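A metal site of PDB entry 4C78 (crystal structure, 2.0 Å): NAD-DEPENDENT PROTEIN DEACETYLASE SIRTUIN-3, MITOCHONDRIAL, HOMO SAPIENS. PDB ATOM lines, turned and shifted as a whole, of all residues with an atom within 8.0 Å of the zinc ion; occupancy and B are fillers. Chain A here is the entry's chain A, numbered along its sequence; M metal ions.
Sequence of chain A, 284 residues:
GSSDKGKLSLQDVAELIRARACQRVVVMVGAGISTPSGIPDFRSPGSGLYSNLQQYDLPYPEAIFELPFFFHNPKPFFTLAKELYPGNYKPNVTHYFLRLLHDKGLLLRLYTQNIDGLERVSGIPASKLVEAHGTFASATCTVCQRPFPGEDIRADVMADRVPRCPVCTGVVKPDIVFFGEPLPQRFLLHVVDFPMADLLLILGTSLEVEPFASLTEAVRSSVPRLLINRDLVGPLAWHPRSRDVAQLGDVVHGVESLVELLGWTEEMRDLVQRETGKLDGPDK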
ATOM      1  N   THR A 140      33.694  -7.075  26.466  1.00  0.00           N
ATOM      2  CA  THR A 140      33.057  -6.266  27.489  1.00  0.00           C
ATOM      3  C   THR A 140      32.072  -5.271  26.841  1.00  0.00           C
ATOM      4  O   THR A 140      32.370  -4.609  25.850  1.00  0.00           O
ATOM      5  CB  THR A 140      34.108  -5.532  28.381  1.00  0.00           C
ATOM      6  OG1 THR A 140      34.905  -6.525  29.074  1.00  0.00           O
ATOM      7  CG2 THR A 140      33.422  -4.673  29.463  1.00  0.00           C
ATOM      8  N   CYS A 141      30.864  -5.210  27.401  1.00  0.00           N
ATOM      9  CA  CYS A 141      29.906  -4.209  26.929  1.00  0.00           C
ATOM     10  C   CYS A 141      30.450  -2.826  27.223  1.00  0.00           C
ATOM     11  O   CYS A 141      30.735  -2.484  28.375  1.00  0.00           O
ATOM     12  CB  CYS A 141      28.564  -4.358  27.609  1.00  0.00           C
ATOM     13  SG  CYS A 141      27.399  -3.154  26.972  1.00  0.00           S
ATOM     14  N   THR A 142      30.556  -2.013  26.185  1.00  0.00           N
ATOM     15  CA  THR A 142      31.070  -0.662  26.317  1.00  0.00           C
ATOM     16  C   THR A 142      30.210   0.229  27.151  1.00  0.00           C
ATOM     17  O   THR A 142      30.620   1.321  27.493  1.00  0.00           O
ATOM     18  CB  THR A 142      31.209   0.030  24.952  1.00  0.00           C
ATOM     19  OG1 THR A 142      29.915   0.079  24.305  1.00  0.00           O
ATOM     20  CG2 THR A 142      32.191  -0.658  24.130  1.00  0.00           C
ATOM     21  N   VAL A 143      28.983  -0.186  27.423  1.00  0.00           N
ATOM     22  CA  VAL A 143      28.072   0.665  28.136  1.00  0.00           C
ATOM     23  C   VAL A 143      27.852   0.154  29.562  1.00  0.00           C
ATOM     24  O   VAL A 143      28.031   0.914  30.478  1.00  0.00           O
ATOM     25  CB  VAL A 143      26.744   0.799  27.356  1.00  0.00           C
ATOM     26  CG1 VAL A 143      25.700   1.381  28.232  1.00  0.00           C
ATOM     27  CG2 VAL A 143      26.957   1.691  26.114  1.00  0.00           C
ATOM     28  N   CYS A 144      27.451  -1.094  29.750  1.00  0.00           N
ATOM     29  CA  CYS A 144      27.065  -1.594  31.086  1.00  0.00           C
ATOM     30  C   CYS A 144      28.151  -2.435  31.707  1.00  0.00           C
ATOM     31  O   CYS A 144      28.048  -2.830  32.861  1.00  0.00           O
ATOM     32  CB  CYS A 144      25.758  -2.369  31.036  1.00  0.00           C
ATOM     33  SG  CYS A 144      25.957  -4.042  30.386  1.00  0.00           S
ATOM     34  N   GLN A 145      29.163  -2.727  30.918  1.00  0.00           N
ATOM     35  CA  GLN A 145      30.411  -3.362  31.351  1.00  0.00           C
ATOM     36  C   GLN A 145      30.243  -4.846  31.604  1.00  0.00           C
ATOM     37  O   GLN A 145      31.168  -5.484  32.032  1.00  0.00           O
ATOM     38  CB  GLN A 145      31.053  -2.637  32.550  1.00  0.00           C
ATOM     39  CG  GLN A 145      31.157  -1.129  32.405  1.00  0.00           C
ATOM     40  CD  GLN A 145      31.899  -0.720  31.144  1.00  0.00           C
ATOM     41  OE1 GLN A 145      32.856  -1.362  30.769  1.00  0.00           O
ATOM     42  NE2 GLN A 145      31.457   0.337  30.464  1.00  0.00           N
ATOM     43  N   ARG A 146      29.060  -5.398  31.350  1.00  0.00           N
ATOM     44  CA  ARG A 146      28.913  -6.860  31.383  1.00  0.00           C
ATOM     45  C   ARG A 146      30.031  -7.519  30.540  1.00  0.00           C
ATOM     46  O   ARG A 146      30.235  -7.143  29.407  1.00  0.00           O
ATOM     47  CB  ARG A 146      27.527  -7.290  30.870  1.00  0.00           C
ATOM     48  CG  ARG A 146      27.335  -8.792  30.712  1.00  0.00           C
ATOM     49  CD  ARG A 146      25.888  -9.161  30.448  1.00  0.00           C
ATOM     50  NE  ARG A 146      25.613 -10.554  30.757  1.00  0.00           N
ATOM     51  CZ  ARG A 146      24.753 -11.008  31.680  1.00  0.00           C
ATOM     52  NH1 ARG A 146      24.017 -10.194  32.449  1.00  0.00           N
ATOM     53  NH2 ARG A 146      24.619 -12.294  31.822  1.00  0.00           N
ATOM     54  N   PRO A 147      30.748  -8.504  31.112  1.00  0.00           N
ATOM     55  CA  PRO A 147      31.755  -9.296  30.412  1.00  0.00           C
ATOM     56  C   PRO A 147      31.151 -10.445  29.610  1.00  0.00           C
ATOM     57  O   PRO A 147      30.037 -10.903  29.937  1.00  0.00           O
ATOM     58  CB  PRO A 147      32.601  -9.857  31.540  1.00  0.00           C
ATOM     59  CG  PRO A 147      31.716  -9.929  32.705  1.00  0.00           C
ATOM     60  CD  PRO A 147      30.712  -8.804  32.550  1.00  0.00           C
ATOM     61  N   PHE A 148      31.808 -10.846  28.535  1.00  0.00           N
ATOM     62  CA  PHE A 148      31.324 -11.919  27.723  1.00  0.00           C
ATOM     63  C   PHE A 148      32.506 -12.776  27.345  1.00  0.00           C
ATOM     64  O   PHE A 148      33.572 -12.267  27.076  1.00  0.00           O
ATOM     65  CB  PHE A 148      30.688 -11.466  26.422  1.00  0.00           C
ATOM     66  CG  PHE A 148      29.423 -10.693  26.592  1.00  0.00           C
ATOM     67  CD1 PHE A 148      29.457  -9.346  26.853  1.00  0.00           C
ATOM     68  CD2 PHE A 148      28.197 -11.326  26.455  1.00  0.00           C
ATOM     69  CE1 PHE A 148      28.289  -8.610  26.962  1.00  0.00           C
ATOM     70  CE2 PHE A 148      27.021 -10.623  26.595  1.00  0.00           C
ATOM     71  CZ  PHE A 148      27.057  -9.249  26.841  1.00  0.00           C
ATOM     72  N   ARG A 164      26.058  -6.625  19.865  1.00  0.00           N
ATOM     73  CA  ARG A 164      25.301  -5.778  20.802  1.00  0.00           C
ATOM     74  C   ARG A 164      24.985  -6.502  22.091  1.00  0.00           C
ATOM     75  O   ARG A 164      24.762  -7.687  22.098  1.00  0.00           O
ATOM     76  CB  ARG A 164      24.007  -5.365  20.164  1.00  0.00           C
ATOM     77  CG  ARG A 164      24.224  -4.769  18.796  1.00  0.00           C
ATOM     78  CD  ARG A 164      23.760  -3.362  18.776  1.00  0.00           C
ATOM     79  NE  ARG A 164      24.377  -2.643  17.670  1.00  0.00           N
ATOM     80  CZ  ARG A 164      24.754  -1.367  17.733  1.00  0.00           C
ATOM     81  NH1 ARG A 164      24.604  -0.653  18.863  1.00  0.00           N
ATOM     82  NH2 ARG A 164      25.317  -0.817  16.668  1.00  0.00           N
ATOM     83  N   CYS A 165      24.956  -5.761  23.181  1.00  0.00           N
ATOM     84  CA  CYS A 165      24.699  -6.338  24.474  1.00  0.00           C
ATOM     85  C   CYS A 165      23.200  -6.756  24.598  1.00  0.00           C
ATOM     86  O   CYS A 165      22.300  -5.991  24.247  1.00  0.00           O
ATOM     87  CB  CYS A 165      25.038  -5.309  25.534  1.00  0.00           C
ATOM     88  SG  CYS A 165      24.979  -5.791  27.244  1.00  0.00           S
ATOM     89  N   PRO A 166      22.962  -7.989  25.067  1.00  0.00           N
ATOM     90  CA  PRO A 166      21.629  -8.364  25.364  1.00  0.00           C
ATOM     91  C   PRO A 166      21.061  -7.565  26.556  1.00  0.00           C
ATOM     92  O   PRO A 166      19.852  -7.522  26.715  1.00  0.00           O
ATOM     93  CB  PRO A 166      21.728  -9.863  25.684  1.00  0.00           C
ATOM     94  CG  PRO A 166      23.108 -10.079  26.160  1.00  0.00           C
ATOM     95  CD  PRO A 166      23.935  -9.046  25.418  1.00  0.00           C
ATOM     96  N   VAL A 167      21.903  -6.959  27.383  1.00  0.00           N
ATOM     97  CA  VAL A 167      21.373  -6.177  28.499  1.00  0.00           C
ATOM     98  C   VAL A 167      20.900  -4.826  28.008  1.00  0.00           C
ATOM     99  O   VAL A 167      19.760  -4.489  28.204  1.00  0.00           O
ATOM    100  CB  VAL A 167      22.433  -5.904  29.573  1.00  0.00           C
ATOM    101  CG1 VAL A 167      21.812  -5.174  30.751  1.00  0.00           C
ATOM    102  CG2 VAL A 167      23.155  -7.179  29.981  1.00  0.00           C
ATOM    103  N   CYS A 168      21.778  -4.074  27.367  1.00  0.00           N
ATOM    104  CA  CYS A 168      21.564  -2.650  27.124  1.00  0.00           C
ATOM    105  C   CYS A 168      21.610  -2.234  25.680  1.00  0.00           C
ATOM    106  O   CYS A 168      21.389  -1.069  25.385  1.00  0.00           O
ATOM    107  CB  CYS A 168      22.603  -1.872  27.903  1.00  0.00           C
ATOM    108  SG  CYS A 168      24.268  -1.988  27.248  1.00  0.00           S
ATOM    109  N   THR A 169      21.910  -3.180  24.807  1.00  0.00           N
ATOM    110  CA  THR A 169      22.095  -2.971  23.355  1.00  0.00           C
ATOM    111  C   THR A 169      23.355  -2.191  22.961  1.00  0.00           C
ATOM    112  O   THR A 169      23.496  -1.812  21.823  1.00  0.00           O
ATOM    113  CB  THR A 169      20.889  -2.265  22.696  1.00  0.00           C
ATOM    114  OG1 THR A 169      21.072  -0.842  22.794  1.00  0.00           O
ATOM    115  CG2 THR A 169      19.576  -2.699  23.320  1.00  0.00           C
ATOM    116  N   GLY A 170      24.246  -1.954  23.902  1.00  0.00           N
ATOM    117  CA  GLY A 170      25.520  -1.326  23.590  1.00  0.00           C
ATOM    118  C   GLY A 170      26.431  -2.236  22.828  1.00  0.00           C
ATOM    119  O   GLY A 170      26.332  -3.457  22.896  1.00  0.00           O
ATOM    120  N   VAL A 171      27.404  -1.626  22.172  1.00  0.00           N
ATOM    121  CA  VAL A 171      28.351  -2.347  21.396  1.00  0.00           C
ATOM    122  C   VAL A 171      29.204  -3.152  22.357  1.00  0.00           C
ATOM    123  O   VAL A 171      29.617  -2.660  23.413  1.00  0.00           O
ATOM    124  CB  VAL A 171      29.249  -1.383  20.637  1.00  0.00           C
ATOM    125  CG1 VAL A 171      30.397  -2.123  19.960  1.00  0.00           C
ATOM    126  CG2 VAL A 171      28.401  -0.631  19.612  1.00  0.00           C
ATOM    127  N   VAL A 172      29.441  -4.405  21.989  1.00  0.00           N
ATOM    128  CA  VAL A 172      30.233  -5.280  22.802  1.00  0.00           C
ATOM    129  C   VAL A 172      31.655  -5.331  22.233  1.00  0.00           C
ATOM    130  O   VAL A 172      31.847  -5.756  21.101  1.00  0.00           O
ATOM    131  CB  VAL A 172      29.682  -6.701  22.828  1.00  0.00           C
ATOM    132  CG1 VAL A 172      30.633  -7.584  23.603  1.00  0.00           C
ATOM    133  CG2 VAL A 172      28.294  -6.717  23.452  1.00  0.00           C
HETATM  134 ZN    ZN M   1      25.494  -3.699  28.129  1.00  0.00          ZN
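The zinc ion is bound by the side-chain sulfur of Cys 168 (2.3 Å), the side-chain sulfur of Cys 141 (2.3 Å), the side-chain sulfur of Cys 165 (2.3 Å) and the side-chain sulfur of Cys 144 (2.3 Å).
Four residues have an atom within 4 Å of the zinc ion: Cys 141, Cys 144, Cys 165 and Cys 168.
SG of Cys 168 lies close to N of Gly 170, 3.3 Å away.
The backbone carbonyl oxygen of Cys 141 lies close to the side-chain amide oxygen of Gln 145.
The side-chain sulfur (SG) of Cys 141 sits close to the backbone NH (N) of Val 143.
The backbone carbonyl oxygen (O) of Arg 146 sits at hydrogen-bond distance from the backbone NH (N) of Cys 141.
N of Val 167 lies close to SG of Cys 165, at 3.3 Å.
The backbone carbonyl oxygen of Gly 170 sits at hydrogen-bond distance from the backbone NH of Cys 165 (2.7 Å).
SG of Cys 144 sits close to N of Arg 146, 3.5 Å away.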
